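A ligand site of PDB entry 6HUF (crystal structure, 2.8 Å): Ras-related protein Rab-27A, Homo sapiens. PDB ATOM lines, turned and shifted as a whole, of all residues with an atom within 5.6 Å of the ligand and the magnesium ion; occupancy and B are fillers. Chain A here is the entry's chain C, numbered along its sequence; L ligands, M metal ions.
N of Thr 23 is in hydrogen-bond range of O7 of the ligand. The backbone NH of Thr 41 sits at hydrogen-bond distance from an oxygen (O2) of the ligand (3.4 Å). N of Ser 24 is in hydrogen-bond range of O7 of the ligand, 3.0 Å away. An oxygen (O7) of the ligand lies within hydrogen-bond range of the side-chain hydroxyl (OG) of Ser 24. N of Ala 154 lies within hydrogen-bond range of O13 of the ligand, 2.9 Å away. The side-chain carboxylate (OD2) of Asp 126 sits at hydrogen-bond distance from a nitrogen (N5) of the ligand, 3.0 Å away. The backbone NH of Gly 67 is in hydrogen-bond range of an oxygen (O3) of the ligand (3.0 Å). The backbone NH of Lys 22 sits close to an oxygen (O4) of the ligand, at 3.3 Å. An oxygen (O3) of the ligand is in salt-bridge range of the side-chain amino group of Lys 22, 3.8 Å away. O12 of the ligand sits at hydrogen-bond distance from O of Ser 36 (3.1 Å). ND2 of Asn 123 lies within hydrogen-bond range of N3 of the ligand. N of Gly 21 sits close to O6 of the ligand (3.3 Å). The backbone NH of Gly 19 lies within hydrogen-bond range of an oxygen (O5) of the ligand. An oxygen (O13) of the ligand sits close to the backbone NH (N) of Lys 124 (3.4 Å). The side-chain hydroxyl (OG) of Ser 18 lies within hydrogen-bond range of an oxygen (O2) of the ligand. N of Val 20 lies within hydrogen-bond range of O5 of the ligand. The side-chain hydroxyl (OG) of Ser 153 lies close to an oxygen (O13) of the ligand, at 3.5 Å.
The side-chain hydroxyl (OG1) of Thr 23 sits close to the side-chain carboxylate (OD2) of Asp 64, at 2.9 Å. The side-chain carboxylate (OD1) of Asp 126 sits at hydrogen-bond distance from the side-chain hydroxyl (OG) of Ser 153, 2.7 Å away. NZ of Lys 22 lies within hydrogen-bond range of O of Gly 16. ND2 of Asn 123 is in hydrogen-bond range of O of Val 20. The side-chain amide oxygen (OD1) of Asn 123 lies within hydrogen-bond range of the side-chain hydroxyl (OG1) of Thr 152. N of Lys 124 is in hydrogen-bond range of O of Thr 152 (3.2 Å). The side-chain hydroxyl (OG) of Ser 153 sits close to the backbone NH (N) of Ala 155.
An oxygen (O5) of the ligand sits close to the backbone carbonyl oxygen of Asp 17 (3.4 Å). CZ of Phe 34 touches O12 of the ligand, at 3.6 Å. Phe 38 touches the ligand. Thr 40 touches the ligand (CA to O2, 3.5 Å). Thr 65 touches the ligand (O to O1, 3.5 Å). Leu 127 touches the ligand. Ala 155 touches the ligand. Hydrophobic or aromatic side chains within 4 Å of the ligand: Phe 34, Phe 38, Leu 127, Ala 154 and Ala 155. 22 residues have an atom within 4 Å of the ligand: Asp 17, Ser 18, Gly 19, Val 20, Gly 21, Lys 22, Thr 23, Ser 24, Phe 34, Ser 36, Phe 38, Thr 40, Thr 41, Thr 65, Gly 67, Asn 123, Lys 124, Asp 126, Leu 127, Ser 153, Ala 154 and Ala 155. The nearest printed residue that does not touch the ligand is Ala 66 (4.1 Å).
Merely in contact with the magnesium ion: Asp 64 (3.4 Å) and Thr 65 (3.96 Å). Four residues have an atom within 4 Å of the magnesium ion: Thr 23, Thr 41, Asp 64 and Thr 65.
The magnesium ion is bound by O1 of the ligand (1.7 Å), OG1 of Thr 23 (1.8 Å), O4 of the ligand (2.3 Å) and OG1 of Thr 41 (2.4 Å). The magnesium ion has four donor atoms within binding distance.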
ATOM      1  N   GLY A  16     -16.967 -20.855  34.186  1.00  0.00           N
ATOM      2  CA  GLY A  16     -15.765 -20.054  34.481  1.00  0.00           C
ATOM      3  C   GLY A  16     -15.623 -18.984  33.410  1.00  0.00           C
ATOM      4  O   GLY A  16     -16.579 -18.780  32.673  1.00  0.00           O
ATOM      5  N   ASP A  17     -14.439 -18.374  33.325  1.00  0.00           N
ATOM      6  CA  ASP A  17     -14.177 -17.207  32.445  1.00  0.00           C
ATOM      7  C   ASP A  17     -13.716 -17.706  31.085  1.00  0.00           C
ATOM      8  O   ASP A  17     -13.404 -18.881  30.972  1.00  0.00           O
ATOM      9  CB  ASP A  17     -13.211 -16.232  33.126  1.00  0.00           C
ATOM     10  CG  ASP A  17     -13.784 -15.584  34.381  1.00  0.00           C
ATOM     11  OD1 ASP A  17     -14.919 -15.968  34.789  1.00  0.00           O
ATOM     12  OD2 ASP A  17     -13.112 -14.686  34.911  1.00  0.00           O
ATOM     13  N   SER A  18     -13.735 -16.832  30.090  1.00  0.00           N
ATOM     14  CA  SER A  18     -13.224 -17.089  28.718  1.00  0.00           C
ATOM     15  C   SER A  18     -11.703 -17.250  28.786  1.00  0.00           C
ATOM     16  O   SER A  18     -11.029 -16.311  29.280  1.00  0.00           O
ATOM     17  CB  SER A  18     -13.645 -15.974  27.791  1.00  0.00           C
ATOM     18  OG  SER A  18     -13.399 -16.287  26.439  1.00  0.00           O
ATOM     19  N   GLY A  19     -11.177 -18.406  28.339  1.00  0.00           N
ATOM     20  CA  GLY A  19      -9.734 -18.672  28.217  1.00  0.00           C
ATOM     21  C   GLY A  19      -9.228 -19.668  29.250  1.00  0.00           C
ATOM     22  O   GLY A  19      -8.073 -20.147  29.127  1.00  0.00           O
ATOM     23  N   VAL A  20     -10.069 -19.952  30.245  1.00  0.00           N
ATOM     24  CA  VAL A  20      -9.775 -20.897  31.350  1.00  0.00           C
ATOM     25  C   VAL A  20      -9.305 -22.218  30.741  1.00  0.00           C
ATOM     26  O   VAL A  20      -8.179 -22.645  31.035  1.00  0.00           O
ATOM     27  CB  VAL A  20     -11.016 -21.087  32.243  1.00  0.00           C
ATOM     28  CG1 VAL A  20     -10.929 -22.349  33.062  1.00  0.00           C
ATOM     29  CG2 VAL A  20     -11.245 -19.882  33.146  1.00  0.00           C
ATOM     30  N   GLY A  21     -10.153 -22.830  29.916  1.00  0.00           N
ATOM     31  CA  GLY A  21      -9.861 -24.052  29.145  1.00  0.00           C
ATOM     32  C   GLY A  21     -10.901 -25.131  29.376  1.00  0.00           C
ATOM     33  O   GLY A  21     -10.515 -26.304  29.355  1.00  0.00           O
ATOM     34  N   LYS A  22     -12.171 -24.771  29.549  1.00  0.00           N
ATOM     35  CA  LYS A  22     -13.257 -25.718  29.950  1.00  0.00           C
ATOM     36  C   LYS A  22     -13.719 -26.526  28.732  1.00  0.00           C
ATOM     37  O   LYS A  22     -14.334 -27.593  28.933  1.00  0.00           O
ATOM     38  CB  LYS A  22     -14.424 -24.989  30.612  1.00  0.00           C
ATOM     39  CG  LYS A  22     -14.697 -23.601  30.067  1.00  0.00           C
ATOM     40  CD  LYS A  22     -15.870 -22.918  30.685  1.00  0.00           C
ATOM     41  CE  LYS A  22     -16.031 -21.536  30.090  1.00  0.00           C
ATOM     42  NZ  LYS A  22     -16.724 -20.645  31.053  1.00  0.00           N
ATOM     43  N   THR A  23     -13.435 -26.054  27.519  1.00  0.00           N
ATOM     44  CA  THR A  23     -13.697 -26.797  26.262  1.00  0.00           C
ATOM     45  C   THR A  23     -12.580 -27.827  26.085  1.00  0.00           C
ATOM     46  O   THR A  23     -12.878 -28.986  25.761  1.00  0.00           O
ATOM     47  CB  THR A  23     -13.800 -25.860  25.056  1.00  0.00           C
ATOM     48  OG1 THR A  23     -14.612 -24.733  25.417  1.00  0.00           O
ATOM     49  CG2 THR A  23     -14.383 -26.538  23.844  1.00  0.00           C
ATOM     50  N   SER A  24     -11.334 -27.401  26.290  1.00  0.00           N
ATOM     51  CA  SER A  24     -10.123 -28.236  26.146  1.00  0.00           C
ATOM     52  C   SER A  24     -10.147 -29.343  27.219  1.00  0.00           C
ATOM     53  O   SER A  24      -9.710 -30.477  26.914  1.00  0.00           O
ATOM     54  CB  SER A  24      -8.889 -27.389  26.185  1.00  0.00           C
ATOM     55  OG  SER A  24      -8.983 -26.348  25.205  1.00  0.00           O
ATOM     56  N   VAL A  25     -10.707 -29.022  28.390  1.00  0.00           N
ATOM     57  CA  VAL A  25     -10.741 -29.916  29.587  1.00  0.00           C
ATOM     58  C   VAL A  25     -11.772 -31.020  29.368  1.00  0.00           C
ATOM     59  O   VAL A  25     -11.463 -32.162  29.684  1.00  0.00           O
ATOM     60  CB  VAL A  25     -11.028 -29.140  30.892  1.00  0.00           C
ATOM     61  CG1 VAL A  25     -11.582 -30.025  32.007  1.00  0.00           C
ATOM     62  CG2 VAL A  25      -9.788 -28.401  31.367  1.00  0.00           C
ATOM     63  N   PHE A  34      -5.774 -33.793  23.422  1.00  0.00           N
ATOM     64  CA  PHE A  34      -5.783 -32.320  23.531  1.00  0.00           C
ATOM     65  C   PHE A  34      -5.839 -31.688  22.132  1.00  0.00           C
ATOM     66  O   PHE A  34      -4.830 -31.798  21.413  1.00  0.00           O
ATOM     67  CB  PHE A  34      -4.531 -31.886  24.299  1.00  0.00           C
ATOM     68  CG  PHE A  34      -4.334 -30.402  24.448  1.00  0.00           C
ATOM     69  CD1 PHE A  34      -5.318 -29.615  25.033  1.00  0.00           C
ATOM     70  CD2 PHE A  34      -3.171 -29.791  23.994  1.00  0.00           C
ATOM     71  CE1 PHE A  34      -5.147 -28.251  25.151  1.00  0.00           C
ATOM     72  CE2 PHE A  34      -3.007 -28.420  24.099  1.00  0.00           C
ATOM     73  CZ  PHE A  34      -4.004 -27.654  24.665  1.00  0.00           C
ATOM     74  N   ASN A  35      -6.976 -31.079  21.761  1.00  0.00           N
ATOM     75  CA  ASN A  35      -7.095 -30.151  20.602  1.00  0.00           C
ATOM     76  C   ASN A  35      -6.673 -28.773  21.116  1.00  0.00           C
ATOM     77  O   ASN A  35      -7.373 -28.246  22.002  1.00  0.00           O
ATOM     78  CB  ASN A  35      -8.498 -30.100  19.984  1.00  0.00           C
ATOM     79  N   SER A  36      -5.566 -28.236  20.617  1.00  0.00           N
ATOM     80  CA  SER A  36      -5.091 -26.880  20.980  1.00  0.00           C
ATOM     81  C   SER A  36      -5.951 -25.828  20.275  1.00  0.00           C
ATOM     82  O   SER A  36      -6.024 -24.698  20.788  1.00  0.00           O
ATOM     83  CB  SER A  36      -3.613 -26.708  20.713  1.00  0.00           C
ATOM     84  OG  SER A  36      -3.285 -26.960  19.357  1.00  0.00           O
ATOM     85  N   LYS A  37      -6.598 -26.186  19.156  1.00  0.00           N
ATOM     86  CA  LYS A  37      -7.558 -25.303  18.429  1.00  0.00           C
ATOM     87  C   LYS A  37      -8.897 -25.319  19.172  1.00  0.00           C
ATOM     88  O   LYS A  37      -9.394 -26.390  19.525  1.00  0.00           O
ATOM     89  CB  LYS A  37      -7.668 -25.723  16.966  1.00  0.00           C
ATOM     90  N   PHE A  38      -9.441 -24.151  19.497  1.00  0.00           N
ATOM     91  CA  PHE A  38     -10.803 -24.021  20.055  1.00  0.00           C
ATOM     92  C   PHE A  38     -11.227 -22.570  19.869  1.00  0.00           C
ATOM     93  O   PHE A  38     -10.587 -21.671  20.447  1.00  0.00           O
ATOM     94  CB  PHE A  38     -10.844 -24.505  21.501  1.00  0.00           C
ATOM     95  N   ILE A  39     -12.205 -22.359  19.003  1.00  0.00           N
ATOM     96  CA  ILE A  39     -12.872 -21.045  18.839  1.00  0.00           C
ATOM     97  C   ILE A  39     -13.444 -20.694  20.216  1.00  0.00           C
ATOM     98  O   ILE A  39     -13.912 -21.612  20.907  1.00  0.00           O
ATOM     99  CB  ILE A  39     -13.933 -21.120  17.709  1.00  0.00           C
ATOM    100  N   THR A  40     -13.306 -19.438  20.651  1.00  0.00           N
ATOM    101  CA  THR A  40     -13.917 -18.952  21.904  1.00  0.00           C
ATOM    102  C   THR A  40     -15.431 -19.187  21.747  1.00  0.00           C
ATOM    103  O   THR A  40     -16.082 -18.393  21.078  1.00  0.00           O
ATOM    104  CB  THR A  40     -13.532 -17.490  22.214  1.00  0.00           C
ATOM    105  OG1 THR A  40     -13.995 -16.658  21.163  1.00  0.00           O
ATOM    106  CG2 THR A  40     -12.048 -17.267  22.352  1.00  0.00           C
ATOM    107  N   THR A  41     -15.899 -20.333  22.255  1.00  0.00           N
ATOM    108  CA  THR A  41     -17.310 -20.813  22.287  1.00  0.00           C
ATOM    109  C   THR A  41     -18.353 -19.705  22.211  1.00  0.00           C
ATOM    110  O   THR A  41     -18.335 -18.809  23.093  1.00  0.00           O
ATOM    111  CB  THR A  41     -17.553 -21.573  23.591  1.00  0.00           C
ATOM    112  OG1 THR A  41     -16.626 -22.661  23.662  1.00  0.00           O
ATOM    113  CG2 THR A  41     -18.974 -22.057  23.751  1.00  0.00           C
ATOM    114  N   ASP A  64     -20.887 -27.697  28.224  1.00  0.00           N
ATOM    115  CA  ASP A  64     -19.918 -26.584  28.073  1.00  0.00           C
ATOM    116  C   ASP A  64     -20.746 -25.309  27.991  1.00  0.00           C
ATOM    117  O   ASP A  64     -21.911 -25.373  27.560  1.00  0.00           O
ATOM    118  CB  ASP A  64     -19.031 -26.820  26.841  1.00  0.00           C
ATOM    119  CG  ASP A  64     -17.771 -25.982  26.730  1.00  0.00           C
ATOM    120  OD1 ASP A  64     -17.707 -24.899  27.353  1.00  0.00           O
ATOM    121  OD2 ASP A  64     -16.860 -26.415  25.991  1.00  0.00           O
ATOM    122  N   THR A  65     -20.172 -24.179  28.424  1.00  0.00           N
ATOM    123  CA  THR A  65     -20.819 -22.837  28.383  1.00  0.00           C
ATOM    124  C   THR A  65     -19.877 -21.844  27.705  1.00  0.00           C
ATOM    125  O   THR A  65     -18.658 -22.138  27.597  1.00  0.00           O
ATOM    126  CB  THR A  65     -21.216 -22.369  29.785  1.00  0.00           C
ATOM    127  OG1 THR A  65     -20.093 -22.393  30.659  1.00  0.00           O
ATOM    128  CG2 THR A  65     -22.302 -23.226  30.389  1.00  0.00           C
ATOM    129  N   ALA A  66     -20.454 -20.739  27.253  1.00  0.00           N
ATOM    130  CA  ALA A  66     -19.715 -19.566  26.728  1.00  0.00           C
ATOM    131  C   ALA A  66     -19.158 -18.792  27.918  1.00  0.00           C
ATOM    132  O   ALA A  66     -19.951 -18.464  28.856  1.00  0.00           O
ATOM    133  CB  ALA A  66     -20.616 -18.716  25.877  1.00  0.00           C
ATOM    134  N   GLY A  67     -17.857 -18.518  27.900  1.00  0.00           N
ATOM    135  CA  GLY A  67     -17.146 -17.814  28.990  1.00  0.00           C
ATOM    136  C   GLY A  67     -17.505 -16.344  29.071  1.00  0.00           C
ATOM    137  O   GLY A  67     -17.177 -15.736  30.115  1.00  0.00           O
ATOM    138  N   LEU A  68     -18.156 -15.790  28.044  1.00  0.00           N
ATOM    139  CA  LEU A  68     -18.410 -14.332  27.974  1.00  0.00           C
ATOM    140  C   LEU A  68     -19.805 -14.021  28.524  1.00  0.00           C
ATOM    141  O   LEU A  68     -20.378 -13.025  28.062  1.00  0.00           O
ATOM    142  CB  LEU A  68     -18.265 -13.868  26.525  1.00  0.00           C
ATOM    143  CG  LEU A  68     -16.864 -14.029  25.921  1.00  0.00           C
ATOM    144  CD1 LEU A  68     -16.876 -13.633  24.448  1.00  0.00           C
ATOM    145  CD2 LEU A  68     -15.845 -13.183  26.670  1.00  0.00           C
ATOM    146  N   ASN A 123      -6.716 -24.627  36.081  1.00  0.00           N
ATOM    147  CA  ASN A 123      -6.266 -25.266  34.818  1.00  0.00           C
ATOM    148  C   ASN A 123      -4.958 -24.648  34.356  1.00  0.00           C
ATOM    149  O   ASN A 123      -4.495 -23.675  34.969  1.00  0.00           O
ATOM    150  CB  ASN A 123      -7.345 -25.159  33.746  1.00  0.00           C
ATOM    151  CG  ASN A 123      -7.223 -26.245  32.705  1.00  0.00           C
ATOM    152  OD1 ASN A 123      -6.867 -27.366  33.029  1.00  0.00           O
ATOM    153  ND2 ASN A 123      -7.519 -25.907  31.467  1.00  0.00           N
ATOM    154  N   LYS A 124      -4.370 -25.201  33.284  1.00  0.00           N
ATOM    155  CA  LYS A 124      -3.193 -24.654  32.584  1.00  0.00           C
ATOM    156  C   LYS A 124      -1.981 -24.748  33.538  1.00  0.00           C
ATOM    157  O   LYS A 124      -1.133 -23.845  33.529  1.00  0.00           O
ATOM    158  CB  LYS A 124      -3.511 -23.245  32.068  1.00  0.00           C
ATOM    159  N   SER A 125      -1.915 -25.829  34.321  1.00  0.00           N
ATOM    160  CA  SER A 125      -0.860 -26.052  35.336  1.00  0.00           C
ATOM    161  C   SER A 125       0.487 -26.321  34.645  1.00  0.00           C
ATOM    162  O   SER A 125       1.545 -26.032  35.265  1.00  0.00           O
ATOM    163  CB  SER A 125      -1.245 -27.157  36.310  1.00  0.00           C
ATOM    164  OG  SER A 125      -1.144 -28.432  35.689  1.00  0.00           O
ATOM    165  N   ASP A 126       0.440 -26.839  33.422  1.00  0.00           N
ATOM    166  CA  ASP A 126       1.644 -27.106  32.576  1.00  0.00           C
ATOM    167  C   ASP A 126       2.392 -25.792  32.342  1.00  0.00           C
ATOM    168  O   ASP A 126       3.650 -25.825  32.275  1.00  0.00           O
ATOM    169  CB  ASP A 126       1.271 -27.758  31.248  1.00  0.00           C
ATOM    170  CG  ASP A 126       0.182 -27.032  30.476  1.00  0.00           C
ATOM    171  OD1 ASP A 126      -0.905 -26.851  31.050  1.00  0.00           O
ATOM    172  OD2 ASP A 126       0.440 -26.646  29.311  1.00  0.00           O
ATOM    173  N   LEU A 127       1.666 -24.678  32.219  1.00  0.00           N
ATOM    174  CA  LEU A 127       2.261 -23.331  32.022  1.00  0.00           C
ATOM    175  C   LEU A 127       2.930 -22.903  33.334  1.00  0.00           C
ATOM    176  O   LEU A 127       2.517 -21.879  33.925  1.00  0.00           O
ATOM    177  CB  LEU A 127       1.166 -22.354  31.580  1.00  0.00           C
ATOM    178  CG  LEU A 127       0.446 -22.730  30.280  1.00  0.00           C
ATOM    179  CD1 LEU A 127      -0.665 -21.746  29.961  1.00  0.00           C
ATOM    180  CD2 LEU A 127       1.433 -22.799  29.121  1.00  0.00           C
ATOM    181  N   THR A 152      -5.191 -28.782  37.354  1.00  0.00           N
ATOM    182  CA  THR A 152      -5.440 -29.583  36.139  1.00  0.00           C
ATOM    183  C   THR A 152      -4.630 -29.009  34.976  1.00  0.00           C
ATOM    184  O   THR A 152      -4.148 -27.846  35.084  1.00  0.00           O
ATOM    185  CB  THR A 152      -6.945 -29.658  35.837  1.00  0.00           C
ATOM    186  OG1 THR A 152      -7.470 -28.353  35.554  1.00  0.00           O
ATOM    187  CG2 THR A 152      -7.736 -30.257  36.983  1.00  0.00           C
ATOM    188  N   SER A 153      -4.450 -29.820  33.936  1.00  0.00           N
ATOM    189  CA  SER A 153      -3.963 -29.432  32.587  1.00  0.00           C
ATOM    190  C   SER A 153      -4.690 -30.261  31.539  1.00  0.00           C
ATOM    191  O   SER A 153      -4.676 -31.499  31.644  1.00  0.00           O
ATOM    192  CB  SER A 153      -2.462 -29.600  32.472  1.00  0.00           C
ATOM    193  OG  SER A 153      -2.032 -29.348  31.138  1.00  0.00           O
ATOM    194  N   ALA A 154      -5.337 -29.605  30.574  1.00  0.00           N
ATOM    195  CA  ALA A 154      -5.984 -30.257  29.419  1.00  0.00           C
ATOM    196  C   ALA A 154      -4.900 -30.661  28.418  1.00  0.00           C
ATOM    197  O   ALA A 154      -5.180 -31.510  27.545  1.00  0.00           O
ATOM    198  CB  ALA A 154      -6.997 -29.331  28.795  1.00  0.00           C
ATOM    199  N   ALA A 155      -3.712 -30.054  28.527  1.00  0.00           N
ATOM    200  CA  ALA A 155      -2.542 -30.378  27.691  1.00  0.00           C
ATOM    201  C   ALA A 155      -1.921 -31.705  28.158  1.00  0.00           C
ATOM    202  O   ALA A 155      -1.613 -32.522  27.292  1.00  0.00           O
ATOM    203  CB  ALA A 155      -1.558 -29.248  27.731  1.00  0.00           C
HETATM  204  P1  LIG L   1     -14.775 -20.252  26.219  1.00  0.00           P
HETATM  205  O1  LIG L   1     -15.632 -21.470  25.929  1.00  0.00           O
HETATM  206  O2  LIG L   1     -14.963 -19.094  25.267  1.00  0.00           O
HETATM  207  O3  LIG L   1     -15.247 -19.950  27.624  1.00  0.00           O
HETATM  208  N1  LIG L   1     -13.210 -20.727  26.186  1.00  0.00           N
HETATM  209  P2  LIG L   1     -12.724 -21.876  27.242  1.00  0.00           P
HETATM  210  O4  LIG L   1     -13.412 -23.182  26.928  1.00  0.00           O
HETATM  211  O5  LIG L   1     -12.796 -21.311  28.650  1.00  0.00           O
HETATM  212  O6  LIG L   1     -11.183 -22.145  26.904  1.00  0.00           O
HETATM  213  P3  LIG L   1     -10.590 -23.016  25.698  1.00  0.00           P
HETATM  214  O7  LIG L   1     -10.748 -24.455  26.007  1.00  0.00           O
HETATM  215  O8  LIG L   1     -11.227 -22.411  24.480  1.00  0.00           O
HETATM  216  O9  LIG L   1      -9.023 -22.730  25.782  1.00  0.00           O
HETATM  217  C1  LIG L   1      -8.613 -21.411  25.414  1.00  0.00           C
HETATM  218  C2  LIG L   1      -7.161 -21.476  25.040  1.00  0.00           C
HETATM  219  O10 LIG L   1      -6.470 -22.027  26.171  1.00  0.00           O
HETATM  220  C3  LIG L   1      -6.814 -22.372  23.854  1.00  0.00           C
HETATM  221  O11 LIG L   1      -5.788 -21.746  23.091  1.00  0.00           O
HETATM  222  C4  LIG L   1      -6.426 -23.688  24.521  1.00  0.00           C
HETATM  223  O12 LIG L   1      -5.469 -24.499  23.851  1.00  0.00           O
HETATM  224  C5  LIG L   1      -5.758 -23.163  25.778  1.00  0.00           C
HETATM  225  N2  LIG L   1      -5.768 -24.111  26.888  1.00  0.00           N
HETATM  226  C6  LIG L   1      -6.826 -24.612  27.591  1.00  0.00           C
HETATM  227  N3  LIG L   1      -6.465 -25.418  28.567  1.00  0.00           N
HETATM  228  C7  LIG L   1      -5.081 -25.432  28.491  1.00  0.00           C
HETATM  229  C8  LIG L   1      -4.129 -26.116  29.288  1.00  0.00           C
HETATM  230  O13 LIG L   1      -4.327 -26.865  30.267  1.00  0.00           O
HETATM  231  N4  LIG L   1      -2.824 -25.837  28.854  1.00  0.00           N
HETATM  232  C9  LIG L   1      -2.482 -25.037  27.780  1.00  0.00           C
HETATM  233  N5  LIG L   1      -1.173 -24.896  27.509  1.00  0.00           N
HETATM  234  N6  LIG L   1      -3.368 -24.384  27.061  1.00  0.00           N
HETATM  235  C10 LIG L   1      -4.636 -24.637  27.467  1.00  0.00           C
HETATM  236 MG    MG M   1     -15.351 -23.165  25.667  1.00  0.00          MG
